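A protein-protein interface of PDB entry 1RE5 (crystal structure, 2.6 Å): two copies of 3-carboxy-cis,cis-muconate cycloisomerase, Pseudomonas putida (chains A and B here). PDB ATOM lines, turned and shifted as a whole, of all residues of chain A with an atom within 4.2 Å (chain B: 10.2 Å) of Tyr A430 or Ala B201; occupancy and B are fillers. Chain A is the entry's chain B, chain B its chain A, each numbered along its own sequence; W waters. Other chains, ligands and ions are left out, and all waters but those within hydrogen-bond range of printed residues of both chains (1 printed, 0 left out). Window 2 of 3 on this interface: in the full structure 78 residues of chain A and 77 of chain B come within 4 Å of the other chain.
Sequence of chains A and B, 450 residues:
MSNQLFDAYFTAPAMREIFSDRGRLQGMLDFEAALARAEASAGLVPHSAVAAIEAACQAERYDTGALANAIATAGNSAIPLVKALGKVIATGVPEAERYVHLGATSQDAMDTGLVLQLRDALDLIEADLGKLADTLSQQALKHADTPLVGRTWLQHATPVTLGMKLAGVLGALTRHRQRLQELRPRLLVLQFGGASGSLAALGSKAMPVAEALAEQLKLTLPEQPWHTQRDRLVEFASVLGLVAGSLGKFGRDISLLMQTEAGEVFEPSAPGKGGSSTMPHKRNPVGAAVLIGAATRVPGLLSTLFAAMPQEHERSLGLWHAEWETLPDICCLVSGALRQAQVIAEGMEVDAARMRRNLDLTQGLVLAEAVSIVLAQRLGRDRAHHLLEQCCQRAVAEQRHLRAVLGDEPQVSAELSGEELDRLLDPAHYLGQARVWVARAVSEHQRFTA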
ATOM      1  N   THR A 158       7.402  -7.008 -15.922  1.00  0.00           N
ATOM      2  CA  THR A 158       7.374  -5.923 -16.895  1.00  0.00           C
ATOM      3  C   THR A 158       7.219  -6.444 -18.326  1.00  0.00           C
ATOM      4  O   THR A 158       7.595  -7.569 -18.637  1.00  0.00           O
ATOM      5  CB  THR A 158       8.637  -5.058 -16.804  1.00  0.00           C
ATOM      6  OG1 THR A 158       9.794  -5.896 -16.857  1.00  0.00           O
ATOM      7  CG2 THR A 158       8.637  -4.257 -15.516  1.00  0.00           C
ATOM      8  N   PRO A 159       6.652  -5.620 -19.212  1.00  0.00           N
ATOM      9  CA  PRO A 159       6.419  -5.962 -20.613  1.00  0.00           C
ATOM     10  C   PRO A 159       7.615  -6.479 -21.383  1.00  0.00           C
ATOM     11  O   PRO A 159       8.775  -6.209 -21.057  1.00  0.00           O
ATOM     12  CB  PRO A 159       5.884  -4.667 -21.203  1.00  0.00           C
ATOM     13  CG  PRO A 159       5.146  -4.067 -20.060  1.00  0.00           C
ATOM     14  CD  PRO A 159       6.110  -4.287 -18.908  1.00  0.00           C
ATOM     15  N   GLU A 369       6.487   0.256 -11.855  1.00  0.00           N
ATOM     16  CA  GLU A 369       7.858   0.732 -12.010  1.00  0.00           C
ATOM     17  C   GLU A 369       7.985   1.874 -13.019  1.00  0.00           C
ATOM     18  O   GLU A 369       8.719   2.830 -12.784  1.00  0.00           O
ATOM     19  CB  GLU A 369       8.741  -0.450 -12.416  1.00  0.00           C
ATOM     20  CG  GLU A 369      10.118  -0.102 -12.937  1.00  0.00           C
ATOM     21  CD  GLU A 369      10.886  -1.341 -13.390  1.00  0.00           C
ATOM     22  OE1 GLU A 369      11.277  -2.145 -12.522  1.00  0.00           O
ATOM     23  OE2 GLU A 369      11.093  -1.523 -14.613  1.00  0.00           O
ATOM     24  N   ALA A 370       7.259   1.775 -14.130  1.00  0.00           N
ATOM     25  CA  ALA A 370       7.295   2.791 -15.180  1.00  0.00           C
ATOM     26  C   ALA A 370       6.780   4.127 -14.667  1.00  0.00           C
ATOM     27  O   ALA A 370       7.238   5.188 -15.095  1.00  0.00           O
ATOM     28  CB  ALA A 370       6.467   2.340 -16.383  1.00  0.00           C
ATOM     29  N   ASP A 426       0.458   2.516 -20.214  1.00  0.00           N
ATOM     30  CA  ASP A 426       0.340   1.828 -21.492  1.00  0.00           C
ATOM     31  C   ASP A 426       1.595   0.969 -21.657  1.00  0.00           C
ATOM     32  O   ASP A 426       2.717   1.481 -21.641  1.00  0.00           O
ATOM     33  CB  ASP A 426       0.219   2.831 -22.643  1.00  0.00           C
ATOM     34  CG  ASP A 426       0.069   2.152 -23.998  1.00  0.00           C
ATOM     35  OD1 ASP A 426      -0.422   1.008 -24.052  1.00  0.00           O
ATOM     36  OD2 ASP A 426       0.431   2.766 -25.022  1.00  0.00           O
ATOM     37  N   PRO A 427       1.417  -0.355 -21.812  1.00  0.00           N
ATOM     38  CA  PRO A 427       2.517  -1.303 -21.973  1.00  0.00           C
ATOM     39  C   PRO A 427       3.389  -0.975 -23.165  1.00  0.00           C
ATOM     40  O   PRO A 427       4.610  -1.078 -23.094  1.00  0.00           O
ATOM     41  CB  PRO A 427       1.804  -2.635 -22.166  1.00  0.00           C
ATOM     42  CG  PRO A 427       0.496  -2.427 -21.534  1.00  0.00           C
ATOM     43  CD  PRO A 427       0.131  -1.048 -21.952  1.00  0.00           C
ATOM     44  N   ALA A 428       2.757  -0.589 -24.266  1.00  0.00           N
ATOM     45  CA  ALA A 428       3.502  -0.264 -25.476  1.00  0.00           C
ATOM     46  C   ALA A 428       4.584   0.800 -25.253  1.00  0.00           C
ATOM     47  O   ALA A 428       5.477   0.956 -26.083  1.00  0.00           O
ATOM     48  CB  ALA A 428       2.544   0.170 -26.570  1.00  0.00           C
ATOM     49  N   HIS A 429       4.519   1.508 -24.130  1.00  0.00           N
ATOM     50  CA  HIS A 429       5.500   2.550 -23.818  1.00  0.00           C
ATOM     51  C   HIS A 429       6.545   2.133 -22.792  1.00  0.00           C
ATOM     52  O   HIS A 429       7.274   2.972 -22.264  1.00  0.00           O
ATOM     53  CB  HIS A 429       4.796   3.817 -23.319  1.00  0.00           C
ATOM     54  CG  HIS A 429       4.049   4.544 -24.388  1.00  0.00           C
ATOM     55  ND1 HIS A 429       4.683   5.208 -25.416  1.00  0.00           N
ATOM     56  CD2 HIS A 429       2.721   4.665 -24.623  1.00  0.00           C
ATOM     57  CE1 HIS A 429       3.778   5.705 -26.241  1.00  0.00           C
ATOM     58  NE2 HIS A 429       2.579   5.388 -25.782  1.00  0.00           N
ATOM     59  N   TYR A 430       6.615   0.846 -22.495  1.00  0.00           N
ATOM     60  CA  TYR A 430       7.594   0.368 -21.537  1.00  0.00           C
ATOM     61  C   TYR A 430       8.208  -0.932 -22.070  1.00  0.00           C
ATOM     62  O   TYR A 430       8.366  -1.914 -21.345  1.00  0.00           O
ATOM     63  CB  TYR A 430       6.927   0.160 -20.173  1.00  0.00           C
ATOM     64  CG  TYR A 430       7.887   0.281 -19.018  1.00  0.00           C
ATOM     65  CD1 TYR A 430       8.628   1.446 -18.825  1.00  0.00           C
ATOM     66  CD2 TYR A 430       8.085  -0.778 -18.132  1.00  0.00           C
ATOM     67  CE1 TYR A 430       9.548   1.555 -17.779  1.00  0.00           C
ATOM     68  CE2 TYR A 430       9.003  -0.685 -17.080  1.00  0.00           C
ATOM     69  CZ  TYR A 430       9.730   0.485 -16.912  1.00  0.00           C
ATOM     70  OH  TYR A 430      10.644   0.582 -15.890  1.00  0.00           O
ATOM     71  N   LEU A 431       8.553  -0.923 -23.356  1.00  0.00           N
ATOM     72  CA  LEU A 431       9.151  -2.077 -24.015  1.00  0.00           C
ATOM     73  C   LEU A 431      10.676  -2.084 -23.956  1.00  0.00           C
ATOM     74  O   LEU A 431      11.319  -3.002 -24.466  1.00  0.00           O
ATOM     75  CB  LEU A 431       8.693  -2.133 -25.468  1.00  0.00           C
ATOM     76  CG  LEU A 431       7.389  -2.876 -25.764  1.00  0.00           C
ATOM     77  CD1 LEU A 431       6.464  -2.837 -24.586  1.00  0.00           C
ATOM     78  CD2 LEU A 431       6.747  -2.257 -26.986  1.00  0.00           C
ATOM     79  N   GLY A 432      11.253  -1.061 -23.331  1.00  0.00           N
ATOM     80  CA  GLY A 432      12.694  -0.983 -23.208  1.00  0.00           C
ATOM     81  C   GLY A 432      13.422  -1.221 -24.514  1.00  0.00           C
ATOM     82  O   GLY A 432      13.086  -0.632 -25.535  1.00  0.00           O
ATOM     83  N   GLU B  39      26.969   3.453 -14.513  1.00  0.00           N
ATOM     84  CA  GLU B  39      25.793   4.307 -14.532  1.00  0.00           C
ATOM     85  C   GLU B  39      26.161   5.724 -14.139  1.00  0.00           C
ATOM     86  O   GLU B  39      25.462   6.676 -14.486  1.00  0.00           O
ATOM     87  CB  GLU B  39      24.724   3.759 -13.587  1.00  0.00           C
ATOM     88  CG  GLU B  39      24.232   2.381 -13.970  1.00  0.00           C
ATOM     89  CD  GLU B  39      23.170   1.860 -13.037  1.00  0.00           C
ATOM     90  OE1 GLU B  39      23.406   1.846 -11.810  1.00  0.00           O
ATOM     91  OE2 GLU B  39      22.099   1.457 -13.532  1.00  0.00           O
ATOM     92  N   LEU B  44      23.593   8.750 -14.114  1.00  0.00           N
ATOM     93  CA  LEU B  44      22.487   8.187 -13.347  1.00  0.00           C
ATOM     94  C   LEU B  44      22.831   8.063 -11.873  1.00  0.00           C
ATOM     95  O   LEU B  44      21.937   7.945 -11.040  1.00  0.00           O
ATOM     96  CB  LEU B  44      22.089   6.810 -13.894  1.00  0.00           C
ATOM     97  CG  LEU B  44      21.073   6.764 -15.039  1.00  0.00           C
ATOM     98  CD1 LEU B  44      19.781   7.389 -14.567  1.00  0.00           C
ATOM     99  CD2 LEU B  44      21.599   7.510 -16.254  1.00  0.00           C
ATOM    100  N   HIS B 101      22.610  -1.526  -7.202  1.00  0.00           N
ATOM    101  CA  HIS B 101      21.828  -2.474  -7.988  1.00  0.00           C
ATOM    102  C   HIS B 101      20.724  -1.804  -8.815  1.00  0.00           C
ATOM    103  O   HIS B 101      19.699  -2.413  -9.100  1.00  0.00           O
ATOM    104  CB  HIS B 101      21.240  -3.512  -7.024  1.00  0.00           C
ATOM    105  CG  HIS B 101      20.802  -4.781  -7.680  1.00  0.00           C
ATOM    106  ND1 HIS B 101      19.480  -5.056  -7.957  1.00  0.00           N
ATOM    107  CD2 HIS B 101      21.509  -5.848  -8.115  1.00  0.00           C
ATOM    108  CE1 HIS B 101      19.394  -6.239  -8.538  1.00  0.00           C
ATOM    109  NE2 HIS B 101      20.612  -6.740  -8.646  1.00  0.00           N
ATOM    110  N   LEU B 102      20.952  -0.560  -9.223  1.00  0.00           N
ATOM    111  CA  LEU B 102      19.976   0.201 -10.000  1.00  0.00           C
ATOM    112  C   LEU B 102      19.718  -0.283 -11.428  1.00  0.00           C
ATOM    113  O   LEU B 102      20.635  -0.339 -12.249  1.00  0.00           O
ATOM    114  CB  LEU B 102      20.397   1.661 -10.059  1.00  0.00           C
ATOM    115  CG  LEU B 102      19.439   2.567 -10.830  1.00  0.00           C
ATOM    116  CD1 LEU B 102      18.081   2.569 -10.137  1.00  0.00           C
ATOM    117  CD2 LEU B 102      20.011   3.982 -10.900  1.00  0.00           C
ATOM    118  N   GLY B 103      18.458  -0.609 -11.716  1.00  0.00           N
ATOM    119  CA  GLY B 103      18.066  -1.062 -13.041  1.00  0.00           C
ATOM    120  C   GLY B 103      18.358  -2.512 -13.382  1.00  0.00           C
ATOM    121  O   GLY B 103      18.009  -2.982 -14.462  1.00  0.00           O
ATOM    122  N   ALA B 104      18.979  -3.233 -12.458  1.00  0.00           N
ATOM    123  CA  ALA B 104      19.339  -4.622 -12.700  1.00  0.00           C
ATOM    124  C   ALA B 104      18.473  -5.606 -11.939  1.00  0.00           C
ATOM    125  O   ALA B 104      17.917  -5.288 -10.889  1.00  0.00           O
ATOM    126  CB  ALA B 104      20.801  -4.843 -12.331  1.00  0.00           C
ATOM    127  N   THR B 105      18.365  -6.813 -12.472  1.00  0.00           N
ATOM    128  CA  THR B 105      17.589  -7.841 -11.803  1.00  0.00           C
ATOM    129  C   THR B 105      18.571  -8.829 -11.142  1.00  0.00           C
ATOM    130  O   THR B 105      19.762  -8.846 -11.480  1.00  0.00           O
ATOM    131  CB  THR B 105      16.659  -8.555 -12.807  1.00  0.00           C
ATOM    132  OG1 THR B 105      15.883  -9.534 -12.116  1.00  0.00           O
ATOM    133  CG2 THR B 105      17.456  -9.218 -13.907  1.00  0.00           C
ATOM    134  N   ASP B 108      20.963 -10.875 -13.297  1.00  0.00           N
ATOM    135  CA  ASP B 108      22.029 -10.122 -13.957  1.00  0.00           C
ATOM    136  C   ASP B 108      23.286 -10.247 -13.095  1.00  0.00           C
ATOM    137  O   ASP B 108      24.362 -10.594 -13.578  1.00  0.00           O
ATOM    138  CB  ASP B 108      21.680  -8.638 -14.075  1.00  0.00           C
ATOM    139  CG  ASP B 108      20.540  -8.365 -15.050  1.00  0.00           C
ATOM    140  OD1 ASP B 108      20.429  -9.087 -16.071  1.00  0.00           O
ATOM    141  OD2 ASP B 108      19.772  -7.400 -14.793  1.00  0.00           O
ATOM    142  N   PHE B 192      23.060  -8.568 -18.739  1.00  0.00           N
ATOM    143  CA  PHE B 192      22.434  -7.356 -18.235  1.00  0.00           C
ATOM    144  C   PHE B 192      21.119  -7.137 -18.993  1.00  0.00           C
ATOM    145  O   PHE B 192      21.103  -6.589 -20.096  1.00  0.00           O
ATOM    146  CB  PHE B 192      23.396  -6.179 -18.438  1.00  0.00           C
ATOM    147  CG  PHE B 192      22.942  -4.887 -17.812  1.00  0.00           C
ATOM    148  CD1 PHE B 192      22.622  -4.828 -16.458  1.00  0.00           C
ATOM    149  CD2 PHE B 192      22.886  -3.719 -18.563  1.00  0.00           C
ATOM    150  CE1 PHE B 192      22.260  -3.631 -15.864  1.00  0.00           C
ATOM    151  CE2 PHE B 192      22.523  -2.511 -17.968  1.00  0.00           C
ATOM    152  CZ  PHE B 192      22.212  -2.473 -16.620  1.00  0.00           C
ATOM    153  N   GLY B 193      20.017  -7.583 -18.400  1.00  0.00           N
ATOM    154  CA  GLY B 193      18.731  -7.432 -19.059  1.00  0.00           C
ATOM    155  C   GLY B 193      17.624  -6.843 -18.208  1.00  0.00           C
ATOM    156  O   GLY B 193      16.623  -6.375 -18.738  1.00  0.00           O
ATOM    157  N   GLY B 194      17.800  -6.852 -16.894  1.00  0.00           N
ATOM    158  CA  GLY B 194      16.779  -6.310 -16.021  1.00  0.00           C
ATOM    159  C   GLY B 194      15.604  -7.259 -15.850  1.00  0.00           C
ATOM    160  O   GLY B 194      15.531  -8.299 -16.503  1.00  0.00           O
ATOM    161  N   ALA B 195      14.676  -6.877 -14.981  1.00  0.00           N
ATOM    162  CA  ALA B 195      13.497  -7.664 -14.658  1.00  0.00           C
ATOM    163  C   ALA B 195      13.043  -8.667 -15.701  1.00  0.00           C
ATOM    164  O   ALA B 195      12.862  -9.848 -15.384  1.00  0.00           O
ATOM    165  CB  ALA B 195      12.348  -6.737 -14.317  1.00  0.00           C
ATOM    166  N   SER B 196      12.845  -8.208 -16.935  1.00  0.00           N
ATOM    167  CA  SER B 196      12.372  -9.101 -17.982  1.00  0.00           C
ATOM    168  C   SER B 196      13.228  -9.075 -19.235  1.00  0.00           C
ATOM    169  O   SER B 196      12.777  -9.494 -20.305  1.00  0.00           O
ATOM    170  CB  SER B 196      10.918  -8.772 -18.344  1.00  0.00           C
ATOM    171  OG  SER B 196      10.808  -7.510 -18.980  1.00  0.00           O
ATOM    172  N   GLY B 197      14.461  -8.585 -19.096  1.00  0.00           N
ATOM    173  CA  GLY B 197      15.368  -8.523 -20.224  1.00  0.00           C
ATOM    174  C   GLY B 197      15.136  -7.369 -21.187  1.00  0.00           C
ATOM    175  O   GLY B 197      15.776  -7.308 -22.233  1.00  0.00           O
ATOM    176  N   SER B 198      14.228  -6.457 -20.851  1.00  0.00           N
ATOM    177  CA  SER B 198      13.949  -5.319 -21.723  1.00  0.00           C
ATOM    178  C   SER B 198      14.810  -4.115 -21.342  1.00  0.00           C
ATOM    179  O   SER B 198      14.994  -3.189 -22.142  1.00  0.00           O
ATOM    180  CB  SER B 198      12.465  -4.939 -21.659  1.00  0.00           C
ATOM    181  OG  SER B 198      12.082  -4.581 -20.344  1.00  0.00           O
ATOM    182  N   LEU B 199      15.333  -4.137 -20.114  1.00  0.00           N
ATOM    183  CA  LEU B 199      16.179  -3.056 -19.622  1.00  0.00           C
ATOM    184  C   LEU B 199      15.398  -1.735 -19.658  1.00  0.00           C
ATOM    185  O   LEU B 199      15.978  -0.654 -19.666  1.00  0.00           O
ATOM    186  CB  LEU B 199      17.430  -2.982 -20.502  1.00  0.00           C
ATOM    187  CG  LEU B 199      18.845  -2.973 -19.912  1.00  0.00           C
ATOM    188  CD1 LEU B 199      18.951  -3.822 -18.666  1.00  0.00           C
ATOM    189  CD2 LEU B 199      19.802  -3.457 -20.996  1.00  0.00           C
ATOM    190  N   ALA B 200      14.074  -1.838 -19.663  1.00  0.00           N
ATOM    191  CA  ALA B 200      13.203  -0.673 -19.717  1.00  0.00           C
ATOM    192  C   ALA B 200      13.419   0.330 -18.584  1.00  0.00           C
ATOM    193  O   ALA B 200      13.269   1.536 -18.780  1.00  0.00           O
ATOM    194  CB  ALA B 200      11.737  -1.123 -19.740  1.00  0.00           C
ATOM    195  N   ALA B 201      13.770  -0.164 -17.402  1.00  0.00           N
ATOM    196  CA  ALA B 201      13.983   0.705 -16.247  1.00  0.00           C
ATOM    197  C   ALA B 201      15.006   1.816 -16.482  1.00  0.00           C
ATOM    198  O   ALA B 201      14.941   2.874 -15.851  1.00  0.00           O
ATOM    199  CB  ALA B 201      14.402  -0.121 -15.060  1.00  0.00           C
ATOM    200  N   LEU B 202      15.951   1.588 -17.385  1.00  0.00           N
ATOM    201  CA  LEU B 202      16.976   2.589 -17.649  1.00  0.00           C
ATOM    202  C   LEU B 202      16.601   3.531 -18.781  1.00  0.00           C
ATOM    203  O   LEU B 202      17.352   4.442 -19.114  1.00  0.00           O
ATOM    204  CB  LEU B 202      18.314   1.906 -17.962  1.00  0.00           C
ATOM    205  CG  LEU B 202      18.913   1.066 -16.837  1.00  0.00           C
ATOM    206  CD1 LEU B 202      20.180   0.367 -17.300  1.00  0.00           C
ATOM    207  CD2 LEU B 202      19.201   1.966 -15.667  1.00  0.00           C
ATOM    208  N   GLY B 203      15.438   3.318 -19.375  1.00  0.00           N
ATOM    209  CA  GLY B 203      15.025   4.184 -20.462  1.00  0.00           C
ATOM    210  C   GLY B 203      16.049   4.232 -21.578  1.00  0.00           C
ATOM    211  O   GLY B 203      16.575   3.203 -21.990  1.00  0.00           O
ATOM    212  N   SER B 204      16.339   5.432 -22.059  1.00  0.00           N
ATOM    213  CA  SER B 204      17.293   5.632 -23.149  1.00  0.00           C
ATOM    214  C   SER B 204      18.767   5.504 -22.758  1.00  0.00           C
ATOM    215  O   SER B 204      19.631   5.503 -23.624  1.00  0.00           O
ATOM    216  CB  SER B 204      17.060   6.996 -23.797  1.00  0.00           C
ATOM    217  OG  SER B 204      17.163   8.031 -22.832  1.00  0.00           O
ATOM    218  N   LYS B 205      19.054   5.402 -21.463  1.00  0.00           N
ATOM    219  CA  LYS B 205      20.433   5.240 -20.999  1.00  0.00           C
ATOM    220  C   LYS B 205      20.799   3.756 -20.941  1.00  0.00           C
ATOM    221  O   LYS B 205      21.860   3.396 -20.446  1.00  0.00           O
ATOM    222  CB  LYS B 205      20.608   5.832 -19.599  1.00  0.00           C
ATOM    223  CG  LYS B 205      20.348   7.315 -19.500  1.00  0.00           C
ATOM    224  CD  LYS B 205      21.357   8.106 -20.305  1.00  0.00           C
ATOM    225  CE  LYS B 205      21.242   9.594 -20.012  1.00  0.00           C
ATOM    226  NZ  LYS B 205      22.272  10.381 -20.752  1.00  0.00           N
ATOM    227  N   ALA B 206      19.914   2.905 -21.454  1.00  0.00           N
ATOM    228  CA  ALA B 206      20.115   1.456 -21.440  1.00  0.00           C
ATOM    229  C   ALA B 206      21.393   0.992 -22.130  1.00  0.00           C
ATOM    230  O   ALA B 206      22.279   0.420 -21.483  1.00  0.00           O
ATOM    231  CB  ALA B 206      18.909   0.761 -22.055  1.00  0.00           C
ATOM    232  N   MET B 207      21.488   1.221 -23.437  1.00  0.00           N
ATOM    233  CA  MET B 207      22.679   0.808 -24.179  1.00  0.00           C
ATOM    234  C   MET B 207      23.956   1.474 -23.678  1.00  0.00           C
ATOM    235  O   MET B 207      25.007   0.840 -23.584  1.00  0.00           O
ATOM    236  CB  MET B 207      22.504   1.077 -25.672  1.00  0.00           C
ATOM    237  CG  MET B 207      21.552   0.106 -26.334  1.00  0.00           C
ATOM    238  SD  MET B 207      22.016  -1.596 -25.952  1.00  0.00           S
ATOM    239  CE  MET B 207      23.405  -1.818 -27.079  1.00  0.00           C
ATOM    240  N   VAL B 209      24.702   2.488 -20.663  1.00  0.00           N
ATOM    241  CA  VAL B 209      25.125   1.860 -19.420  1.00  0.00           C
ATOM    242  C   VAL B 209      25.613   0.439 -19.673  1.00  0.00           C
ATOM    243  O   VAL B 209      26.572  -0.018 -19.052  1.00  0.00           O
ATOM    244  CB  VAL B 209      23.987   1.824 -18.376  1.00  0.00           C
ATOM    245  CG1 VAL B 209      24.404   0.994 -17.189  1.00  0.00           C
ATOM    246  CG2 VAL B 209      23.673   3.217 -17.911  1.00  0.00           C
HETATM  247  O   HOH W   1      12.988  -5.859 -17.898  1.00  0.00           O
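Water W1 lies within hydrogen-bond range of N of Ser B196 (2.5 Å), OG of Ser B198 (2.9 Å), N of Gly B197 (3.3 Å) and OG1 of Thr A158 (3.4 Å).
Printed residues of chain B that touch a printed residue of chain A: Ala B195, Ser B196, Ser B198, Ala B200 and Ala B201.
Along chain B the printed residues that touch a printed residue of chain A span positions 195 to 201.
Of the 11 printed residues of chain A, 6 touch a printed residue of chain B.
Printed residues of chain A that touch a printed residue of chain B: Thr A158, Pro A159, Glu A369, Tyr A430, Leu A431 and Gly A432.
Hydrophobic or aromatic side chains of chain A within 4 Å of the printed part of chain B: Tyr A430.
Among the printed residues, 10 pairs touch across the chains.
Among the printed residues, no Asp or Glu carboxylate lies within 4 Å of a Lys or Arg side-chain nitrogen of the other chain.
The backbone NH (N) of Ser B198 is in hydrogen-bond range of the backbone carbonyl oxygen (O) of Gly B193.
OG of Ser B196 is in hydrogen-bond range of OG of Ser B198 (3.5 Å).
N of Ala B200 lies close to OG of Ser B198, at 3.5 Å.
The side-chain hydroxyl of Tyr A430 is in hydrogen-bond range of the side-chain carboxylate of Glu A369, 2.5 Å away.
Of chain B, only Ser B196 (3.2 Å) and Ser B198 (3.8 Å) come within 4 Å of Pro A159.
Glu A369 touches just one residue of chain B: Ala B201.
No residue of chain B comes within 4 Å of Ala A370.
No residue of chain B comes within 4 Å of Ala A428.
Tyr A430 touches two residues of chain B.
Leu A431 touches just one residue of chain B: Ser B198 (3.6 Å).
Glu B39 touches none of the printed residues of chain A.
Gly B193 touches none of the printed residues of chain A.
Of the printed residues of chain A, Ser B196 touches Thr A158 and Pro A159.
Of the printed residues of chain A, Ala B200 touches Tyr A430 and Gly A432.
Of chain A, only Glu A369 and Tyr A430 come within 4 Å of Ala B201.
The nearest printed residue of chain A that does not touch Ala B201 is Gly A432 (6.0 Å).
The nearest printed residue of chain A that does not touch Ala B200 is Leu A431 (4.5 Å).
Ala B195 touches Thr A158.
O of Pro A159 touches OG of Ser B198, at 3.8 Å.
Ala B201 touches Glu A369 (CB to OE2, 3.6 Å).
Ala B200 touches Tyr A430.
CA of Ala B201 touches OH of Tyr A430, at 3.4 Å.
Ser B198 touches Leu A431.
Ser B198 touches Gly A432.
Gly A432 touches Ala B200 (CA to CA, 3.5 Å).
OG1 of Thr A158 lies within hydrogen-bond range of OG of Ser B196 (2.9 Å).
The side-chain hydroxyl of Ser B196 is in hydrogen-bond range of the backbone carbonyl oxygen of Pro A159.
No position is printed for both chains.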
